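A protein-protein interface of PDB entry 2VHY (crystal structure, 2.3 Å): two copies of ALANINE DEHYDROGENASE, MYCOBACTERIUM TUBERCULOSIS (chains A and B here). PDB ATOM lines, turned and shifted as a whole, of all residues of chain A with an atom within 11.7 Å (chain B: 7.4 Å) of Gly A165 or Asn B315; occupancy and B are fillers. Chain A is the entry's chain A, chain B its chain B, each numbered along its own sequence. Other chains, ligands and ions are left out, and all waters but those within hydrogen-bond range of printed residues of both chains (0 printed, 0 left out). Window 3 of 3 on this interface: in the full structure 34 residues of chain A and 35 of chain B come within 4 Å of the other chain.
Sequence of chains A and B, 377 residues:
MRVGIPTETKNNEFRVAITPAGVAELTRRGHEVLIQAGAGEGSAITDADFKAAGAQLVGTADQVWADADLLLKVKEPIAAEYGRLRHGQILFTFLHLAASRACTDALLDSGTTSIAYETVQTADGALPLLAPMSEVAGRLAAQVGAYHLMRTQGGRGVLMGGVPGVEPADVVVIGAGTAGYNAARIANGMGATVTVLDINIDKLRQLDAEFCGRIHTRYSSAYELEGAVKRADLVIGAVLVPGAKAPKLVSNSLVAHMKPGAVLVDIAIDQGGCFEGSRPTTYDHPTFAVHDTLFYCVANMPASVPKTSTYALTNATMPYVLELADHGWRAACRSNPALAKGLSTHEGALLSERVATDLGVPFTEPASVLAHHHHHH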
ATOM      1  N   LEU A 159      22.056  -3.564  -9.218  1.00  0.00           N
ATOM      2  CA  LEU A 159      22.046  -4.447 -10.387  1.00  0.00           C
ATOM      3  C   LEU A 159      23.442  -5.051 -10.367  1.00  0.00           C
ATOM      4  O   LEU A 159      24.418  -4.350 -10.105  1.00  0.00           O
ATOM      5  CB  LEU A 159      21.825  -3.666 -11.700  1.00  0.00           C
ATOM      6  CG  LEU A 159      21.632  -4.398 -13.046  1.00  0.00           C
ATOM      7  CD1 LEU A 159      20.485  -5.373 -12.936  1.00  0.00           C
ATOM      8  CD2 LEU A 159      21.346  -3.392 -14.160  1.00  0.00           C
ATOM      9  N   GLY A 161      25.663  -6.015 -12.633  1.00  0.00           N
ATOM     10  CA  GLY A 161      26.712  -5.406 -13.428  1.00  0.00           C
ATOM     11  C   GLY A 161      26.540  -3.940 -13.738  1.00  0.00           C
ATOM     12  O   GLY A 161      27.156  -3.420 -14.668  1.00  0.00           O
ATOM     13  N   GLY A 162      25.716  -3.264 -12.945  1.00  0.00           N
ATOM     14  CA  GLY A 162      25.474  -1.858 -13.178  1.00  0.00           C
ATOM     15  C   GLY A 162      25.061  -1.623 -14.616  1.00  0.00           C
ATOM     16  O   GLY A 162      24.494  -2.504 -15.278  1.00  0.00           O
ATOM     17  N   VAL A 163      25.338  -0.412 -15.082  1.00  0.00           N
ATOM     18  CA  VAL A 163      25.049   0.027 -16.443  1.00  0.00           C
ATOM     19  C   VAL A 163      26.135   1.071 -16.714  1.00  0.00           C
ATOM     20  O   VAL A 163      26.670   1.661 -15.774  1.00  0.00           O
ATOM     21  CB  VAL A 163      23.630   0.686 -16.570  1.00  0.00           C
ATOM     22  CG1 VAL A 163      22.546  -0.348 -16.276  1.00  0.00           C
ATOM     23  CG2 VAL A 163      23.510   1.898 -15.632  1.00  0.00           C
ATOM     24  N   PRO A 164      26.499   1.290 -17.990  1.00  0.00           N
ATOM     25  CA  PRO A 164      27.538   2.279 -18.325  1.00  0.00           C
ATOM     26  C   PRO A 164      27.465   3.553 -17.455  1.00  0.00           C
ATOM     27  O   PRO A 164      26.380   4.120 -17.258  1.00  0.00           O
ATOM     28  CB  PRO A 164      27.262   2.563 -19.795  1.00  0.00           C
ATOM     29  CG  PRO A 164      26.840   1.208 -20.298  1.00  0.00           C
ATOM     30  CD  PRO A 164      25.921   0.693 -19.207  1.00  0.00           C
ATOM     31  N   GLY A 165      28.608   3.990 -16.932  1.00  0.00           N
ATOM     32  CA  GLY A 165      28.627   5.187 -16.109  1.00  0.00           C
ATOM     33  C   GLY A 165      28.168   4.992 -14.670  1.00  0.00           C
ATOM     34  O   GLY A 165      28.288   5.901 -13.830  1.00  0.00           O
ATOM     35  N   VAL A 166      27.628   3.817 -14.375  1.00  0.00           N
ATOM     36  CA  VAL A 166      27.161   3.526 -13.025  1.00  0.00           C
ATOM     37  C   VAL A 166      27.900   2.282 -12.529  1.00  0.00           C
ATOM     38  O   VAL A 166      28.019   1.288 -13.240  1.00  0.00           O
ATOM     39  CB  VAL A 166      25.583   3.385 -12.981  1.00  0.00           C
ATOM     40  CG1 VAL A 166      25.094   2.875 -11.632  1.00  0.00           C
ATOM     41  CG2 VAL A 166      24.972   4.738 -13.225  1.00  0.00           C
ATOM     42  N   GLU A 167      28.423   2.392 -11.308  1.00  0.00           N
ATOM     43  CA  GLU A 167      29.204   1.358 -10.645  1.00  0.00           C
ATOM     44  C   GLU A 167      28.559  -0.028 -10.537  1.00  0.00           C
ATOM     45  O   GLU A 167      27.400  -0.162 -10.152  1.00  0.00           O
ATOM     46  CB  GLU A 167      29.602   1.850  -9.247  1.00  0.00           C
ATOM     47  CG  GLU A 167      30.151   0.750  -8.362  1.00  0.00           C
ATOM     48  CD  GLU A 167      30.686   1.252  -7.038  1.00  0.00           C
ATOM     49  OE1 GLU A 167      29.974   2.024  -6.344  1.00  0.00           O
ATOM     50  OE2 GLU A 167      31.823   0.854  -6.689  1.00  0.00           O
ATOM     51  N   PRO A 168      29.320  -1.085 -10.870  1.00  0.00           N
ATOM     52  CA  PRO A 168      28.778  -2.439 -10.789  1.00  0.00           C
ATOM     53  C   PRO A 168      28.758  -2.961  -9.347  1.00  0.00           C
ATOM     54  O   PRO A 168      29.365  -2.362  -8.453  1.00  0.00           O
ATOM     55  CB  PRO A 168      29.708  -3.226 -11.701  1.00  0.00           C
ATOM     56  CG  PRO A 168      31.010  -2.552 -11.481  1.00  0.00           C
ATOM     57  CD  PRO A 168      30.649  -1.088 -11.508  1.00  0.00           C
ATOM     58  N   ALA A 169      28.046  -4.070  -9.134  1.00  0.00           N
ATOM     59  CA  ALA A 169      27.915  -4.698  -7.818  1.00  0.00           C
ATOM     60  C   ALA A 169      29.209  -5.365  -7.361  1.00  0.00           C
ATOM     61  O   ALA A 169      30.002  -5.846  -8.179  1.00  0.00           O
ATOM     62  CB  ALA A 169      26.785  -5.723  -7.832  1.00  0.00           C
ATOM     63  N   GLY A 191      28.286  -9.161 -14.977  1.00  0.00           N
ATOM     64  CA  GLY A 191      28.882  -7.841 -14.990  1.00  0.00           C
ATOM     65  C   GLY A 191      29.457  -7.406 -13.671  1.00  0.00           C
ATOM     66  O   GLY A 191      30.187  -6.430 -13.611  1.00  0.00           O
ATOM     67  N   THR A 193      31.499  -7.015 -10.056  1.00  0.00           N
ATOM     68  CA  THR A 193      32.901  -6.928  -9.671  1.00  0.00           C
ATOM     69  C   THR A 193      33.137  -8.009  -8.606  1.00  0.00           C
ATOM     70  O   THR A 193      32.856  -7.813  -7.426  1.00  0.00           O
ATOM     71  CB  THR A 193      33.237  -5.536  -9.132  1.00  0.00           C
ATOM     72  OG1 THR A 193      32.984  -4.567 -10.156  1.00  0.00           O
ATOM     73  CG2 THR A 193      34.706  -5.455  -8.751  1.00  0.00           C
ATOM     74  N   ALA B  17      15.553  11.929  -7.584  1.00  0.00           N
ATOM     75  CA  ALA B  17      15.836  12.771  -8.742  1.00  0.00           C
ATOM     76  C   ALA B  17      17.227  13.358  -8.816  1.00  0.00           C
ATOM     77  O   ALA B  17      17.576  13.991  -9.818  1.00  0.00           O
ATOM     78  CB  ALA B  17      14.799  13.894  -8.828  1.00  0.00           C
ATOM     79  N   THR B  19      21.606  13.024  -7.191  1.00  0.00           N
ATOM     80  CA  THR B  19      22.647  12.357  -6.419  1.00  0.00           C
ATOM     81  C   THR B  19      23.588  13.407  -5.841  1.00  0.00           C
ATOM     82  O   THR B  19      23.656  14.530  -6.345  1.00  0.00           O
ATOM     83  CB  THR B  19      23.476  11.395  -7.316  1.00  0.00           C
ATOM     84  OG1 THR B  19      23.994  12.110  -8.448  1.00  0.00           O
ATOM     85  CG2 THR B  19      22.607  10.236  -7.810  1.00  0.00           C
ATOM     86  N   ALA B  21      26.273  13.932  -6.361  1.00  0.00           N
ATOM     87  CA  ALA B  21      27.092  14.341  -7.499  1.00  0.00           C
ATOM     88  C   ALA B  21      26.468  15.544  -8.202  1.00  0.00           C
ATOM     89  O   ALA B  21      27.133  16.558  -8.439  1.00  0.00           O
ATOM     90  CB  ALA B  21      27.229  13.172  -8.477  1.00  0.00           C
ATOM     91  N   GLY B  22      25.185  15.424  -8.538  1.00  0.00           N
ATOM     92  CA  GLY B  22      24.493  16.510  -9.202  1.00  0.00           C
ATOM     93  C   GLY B  22      24.263  17.644  -8.229  1.00  0.00           C
ATOM     94  O   GLY B  22      24.456  18.809  -8.563  1.00  0.00           O
ATOM     95  N   LEU B 129      16.881  10.155 -21.624  1.00  0.00           N
ATOM     96  CA  LEU B 129      16.491   9.827 -20.253  1.00  0.00           C
ATOM     97  C   LEU B 129      15.809   8.468 -20.091  1.00  0.00           C
ATOM     98  O   LEU B 129      15.672   7.964 -18.968  1.00  0.00           O
ATOM     99  CB  LEU B 129      15.635  10.969 -19.667  1.00  0.00           C
ATOM    100  CG  LEU B 129      16.201  12.384 -19.909  1.00  0.00           C
ATOM    101  CD1 LEU B 129      15.343  13.416 -19.189  1.00  0.00           C
ATOM    102  CD2 LEU B 129      17.664  12.467 -19.450  1.00  0.00           C
ATOM    103  N   PRO B 132      18.879   4.857 -20.199  1.00  0.00           N
ATOM    104  CA  PRO B 132      19.351   4.216 -18.961  1.00  0.00           C
ATOM    105  C   PRO B 132      18.361   3.241 -18.362  1.00  0.00           C
ATOM    106  O   PRO B 132      18.727   2.181 -17.858  1.00  0.00           O
ATOM    107  CB  PRO B 132      19.611   5.405 -18.028  1.00  0.00           C
ATOM    108  CG  PRO B 132      18.620   6.432 -18.490  1.00  0.00           C
ATOM    109  CD  PRO B 132      18.769   6.318 -19.999  1.00  0.00           C
ATOM    110  N   GLU B 135      18.332   0.128 -20.202  1.00  0.00           N
ATOM    111  CA  GLU B 135      19.523  -0.644 -19.888  1.00  0.00           C
ATOM    112  C   GLU B 135      19.290  -1.391 -18.592  1.00  0.00           C
ATOM    113  O   GLU B 135      19.537  -2.590 -18.503  1.00  0.00           O
ATOM    114  CB  GLU B 135      20.747   0.275 -19.735  1.00  0.00           C
ATOM    115  CG  GLU B 135      21.109   1.035 -21.003  1.00  0.00           C
ATOM    116  CD  GLU B 135      22.254   2.010 -20.805  1.00  0.00           C
ATOM    117  OE1 GLU B 135      22.658   2.665 -21.793  1.00  0.00           O
ATOM    118  OE2 GLU B 135      22.748   2.121 -19.662  1.00  0.00           O
ATOM    119  N   THR B 308      21.173   1.692  -8.342  1.00  0.00           N
ATOM    120  CA  THR B 308      21.584   1.671  -9.740  1.00  0.00           C
ATOM    121  C   THR B 308      20.821   2.674 -10.592  1.00  0.00           C
ATOM    122  O   THR B 308      21.397   3.636 -11.121  1.00  0.00           O
ATOM    123  CB  THR B 308      21.346   0.286 -10.389  1.00  0.00           C
ATOM    124  OG1 THR B 308      22.074  -0.714  -9.677  1.00  0.00           O
ATOM    125  CG2 THR B 308      21.799   0.292 -11.847  1.00  0.00           C
ATOM    126  N   SER B 309      19.519   2.421 -10.728  1.00  0.00           N
ATOM    127  CA  SER B 309      18.656   3.255 -11.548  1.00  0.00           C
ATOM    128  C   SER B 309      18.666   4.745 -11.216  1.00  0.00           C
ATOM    129  O   SER B 309      18.615   5.564 -12.129  1.00  0.00           O
ATOM    130  CB  SER B 309      17.229   2.707 -11.531  1.00  0.00           C
ATOM    131  OG  SER B 309      16.731   2.658 -10.216  1.00  0.00           O
ATOM    132  N   THR B 310      18.731   5.114  -9.936  1.00  0.00           N
ATOM    133  CA  THR B 310      18.785   6.540  -9.585  1.00  0.00           C
ATOM    134  C   THR B 310      19.964   7.168 -10.305  1.00  0.00           C
ATOM    135  O   THR B 310      19.812   8.157 -11.005  1.00  0.00           O
ATOM    136  CB  THR B 310      18.984   6.771  -8.072  1.00  0.00           C
ATOM    137  OG1 THR B 310      17.774   6.463  -7.385  1.00  0.00           O
ATOM    138  CG2 THR B 310      19.360   8.224  -7.785  1.00  0.00           C
ATOM    139  N   TYR B 311      21.139   6.580 -10.122  1.00  0.00           N
ATOM    140  CA  TYR B 311      22.360   7.066 -10.748  1.00  0.00           C
ATOM    141  C   TYR B 311      22.271   7.025 -12.259  1.00  0.00           C
ATOM    142  O   TYR B 311      22.640   7.971 -12.941  1.00  0.00           O
ATOM    143  CB  TYR B 311      23.526   6.214 -10.271  1.00  0.00           C
ATOM    144  CG  TYR B 311      23.974   6.587  -8.888  1.00  0.00           C
ATOM    145  CD1 TYR B 311      24.949   7.557  -8.703  1.00  0.00           C
ATOM    146  CD2 TYR B 311      23.383   6.012  -7.755  1.00  0.00           C
ATOM    147  CE1 TYR B 311      25.332   7.957  -7.426  1.00  0.00           C
ATOM    148  CE2 TYR B 311      23.756   6.404  -6.469  1.00  0.00           C
ATOM    149  CZ  TYR B 311      24.735   7.383  -6.316  1.00  0.00           C
ATOM    150  OH  TYR B 311      25.142   7.801  -5.069  1.00  0.00           O
ATOM    151  N   ALA B 312      21.772   5.915 -12.778  1.00  0.00           N
ATOM    152  CA  ALA B 312      21.628   5.744 -14.215  1.00  0.00           C
ATOM    153  C   ALA B 312      20.887   6.922 -14.838  1.00  0.00           C
ATOM    154  O   ALA B 312      21.344   7.511 -15.818  1.00  0.00           O
ATOM    155  CB  ALA B 312      20.895   4.450 -14.500  1.00  0.00           C
ATOM    156  N   LEU B 313      19.746   7.270 -14.250  1.00  0.00           N
ATOM    157  CA  LEU B 313      18.925   8.361 -14.748  1.00  0.00           C
ATOM    158  C   LEU B 313      19.413   9.752 -14.385  1.00  0.00           C
ATOM    159  O   LEU B 313      19.447  10.637 -15.243  1.00  0.00           O
ATOM    160  CB  LEU B 313      17.498   8.206 -14.250  1.00  0.00           C
ATOM    161  CG  LEU B 313      16.562   9.279 -14.804  1.00  0.00           C
ATOM    162  CD1 LEU B 313      16.355   9.054 -16.302  1.00  0.00           C
ATOM    163  CD2 LEU B 313      15.241   9.236 -14.055  1.00  0.00           C
ATOM    164  N   THR B 314      19.774   9.969 -13.126  1.00  0.00           N
ATOM    165  CA  THR B 314      20.241  11.289 -12.733  1.00  0.00           C
ATOM    166  C   THR B 314      21.494  11.699 -13.518  1.00  0.00           C
ATOM    167  O   THR B 314      21.782  12.888 -13.677  1.00  0.00           O
ATOM    168  CB  THR B 314      20.503  11.380 -11.209  1.00  0.00           C
ATOM    169  OG1 THR B 314      21.561  10.493 -10.843  1.00  0.00           O
ATOM    170  CG2 THR B 314      19.250  11.017 -10.434  1.00  0.00           C
ATOM    171  N   ASN B 315      22.227  10.720 -14.028  1.00  0.00           N
ATOM    172  CA  ASN B 315      23.420  11.022 -14.813  1.00  0.00           C
ATOM    173  C   ASN B 315      23.036  11.548 -16.181  1.00  0.00           C
ATOM    174  O   ASN B 315      23.775  12.333 -16.789  1.00  0.00           O
ATOM    175  CB  ASN B 315      24.275   9.779 -15.024  1.00  0.00           C
ATOM    176  CG  ASN B 315      25.093   9.422 -13.820  1.00  0.00           C
ATOM    177  OD1 ASN B 315      25.273  10.235 -12.898  1.00  0.00           O
ATOM    178  ND2 ASN B 315      25.617   8.199 -13.821  1.00  0.00           N
ATOM    179  N   ALA B 316      21.891  11.078 -16.668  1.00  0.00           N
ATOM    180  CA  ALA B 316      21.362  11.462 -17.973  1.00  0.00           C
ATOM    181  C   ALA B 316      20.603  12.777 -17.841  1.00  0.00           C
ATOM    182  O   ALA B 316      20.532  13.583 -18.774  1.00  0.00           O
ATOM    183  CB  ALA B 316      20.425  10.356 -18.495  1.00  0.00           C
ATOM    184  N   THR B 317      20.048  12.972 -16.652  1.00  0.00           N
ATOM    185  CA  THR B 317      19.269  14.150 -16.315  1.00  0.00           C
ATOM    186  C   THR B 317      20.137  15.364 -15.989  1.00  0.00           C
ATOM    187  O   THR B 317      19.787  16.500 -16.329  1.00  0.00           O
ATOM    188  CB  THR B 317      18.352  13.824 -15.118  1.00  0.00           C
ATOM    189  OG1 THR B 317      17.208  13.097 -15.586  1.00  0.00           O
ATOM    190  CG2 THR B 317      17.909  15.075 -14.417  1.00  0.00           C
ATOM    191  N   MET B 318      21.267  15.103 -15.335  1.00  0.00           N
ATOM    192  CA  MET B 318      22.205  16.135 -14.919  1.00  0.00           C
ATOM    193  C   MET B 318      22.438  17.289 -15.872  1.00  0.00           C
ATOM    194  O   MET B 318      22.258  18.433 -15.492  1.00  0.00           O
ATOM    195  CB  MET B 318      23.552  15.516 -14.562  1.00  0.00           C
ATOM    196  CG  MET B 318      23.738  15.264 -13.083  1.00  0.00           C
ATOM    197  SD  MET B 318      25.463  15.543 -12.570  1.00  0.00           S
ATOM    198  CE  MET B 318      25.976  13.852 -12.185  1.00  0.00           C
ATOM    199  N   PRO B 319      22.852  17.015 -17.119  1.00  0.00           N
ATOM    200  CA  PRO B 319      23.082  18.134 -18.039  1.00  0.00           C
ATOM    201  C   PRO B 319      21.912  19.070 -18.287  1.00  0.00           C
ATOM    202  O   PRO B 319      22.127  20.263 -18.464  1.00  0.00           O
ATOM    203  CB  PRO B 319      23.576  17.451 -19.321  1.00  0.00           C
ATOM    204  CG  PRO B 319      23.059  16.063 -19.210  1.00  0.00           C
ATOM    205  CD  PRO B 319      23.215  15.738 -17.751  1.00  0.00           C
ATOM    206  N   TYR B 320      20.683  18.545 -18.296  1.00  0.00           N
ATOM    207  CA  TYR B 320      19.491  19.379 -18.527  1.00  0.00           C
ATOM    208  C   TYR B 320      19.063  20.163 -17.290  1.00  0.00           C
ATOM    209  O   TYR B 320      18.686  21.335 -17.378  1.00  0.00           O
ATOM    210  CB  TYR B 320      18.309  18.530 -18.982  1.00  0.00           C
ATOM    211  CG  TYR B 320      18.549  17.817 -20.271  1.00  0.00           C
ATOM    212  CD1 TYR B 320      19.054  16.524 -20.283  1.00  0.00           C
ATOM    213  CD2 TYR B 320      18.298  18.445 -21.492  1.00  0.00           C
ATOM    214  CE1 TYR B 320      19.311  15.865 -21.485  1.00  0.00           C
ATOM    215  CE2 TYR B 320      18.548  17.803 -22.702  1.00  0.00           C
ATOM    216  CZ  TYR B 320      19.057  16.509 -22.694  1.00  0.00           C
ATOM    217  OH  TYR B 320      19.324  15.861 -23.884  1.00  0.00           O
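The backbone NH (N) of Leu A159 lies within hydrogen-bond range of the side-chain hydroxyl (OG1) of Thr B308 (2.9 Å).
Glu B135 touches Val A163 (OE2 to CB, 3.5 Å). Ala B312 touches Val A163. CD of Pro A164 touches OE2 of Glu B135, 3.5 Å away. Asn B315 touches Gly A165 (ND2 to O, 3.5 Å). Thr B308 touches Val A166 (O to CG1, 3.8 Å). Val A166 touches Tyr B311. N of Ala B312 touches CG2 of Val A166 (3.4 Å). Asn B315 touches Val A166.
Hydrophobic or aromatic side chains of chain B within 4 Å of the printed part of chain A: Tyr B311 and Ala B312. Printed residues of chain A that touch a printed residue of chain B: Leu A159, Val A163, Pro A164, Gly A165 and Val A166. Among the printed residues, no Asp or Glu carboxylate lies within 4 Å of a Lys or Arg side-chain nitrogen of the other chain.
The backbone carbonyl oxygen (O) of Tyr B311 lies within hydrogen-bond range of the side-chain hydroxyl (OG1) of Thr B314, at 3.5 Å. The side-chain amide nitrogen (ND2) of Asn B315 sits close to the backbone carbonyl oxygen (O) of Tyr B311 (3.1 Å).
Of the printed residues of chain B, Leu A159 touches Thr B308 (2.9 Å). Printed residues of chain B within 4 Å of Gly A165: Asn B315. Printed residues of chain B within 4 Å of Val A166: Thr B308 (3.8 Å), Tyr B311 (3.6 Å), Ala B312 (3.4 Å) and Asn B315 (3.6 Å). Ala B312 touches just these residues of chain A: Val A163 (3.8 Å) and Val A166 (3.4 Å). No residue of chain A comes within 4 Å of Leu B313. Asn B315 touches two residues of chain A. No residue of chain A comes within 4 Å of Ala B316. No residue of chain A comes within 4 Å of Thr B317. The nearest printed residue of chain A that does not touch Glu B135 is Leu A159 (4.8 Å).
No position is printed for both chains. Of the 9 pairs that touch across the chains among the printed residues, none has its exchanged pair printed and touching as well.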
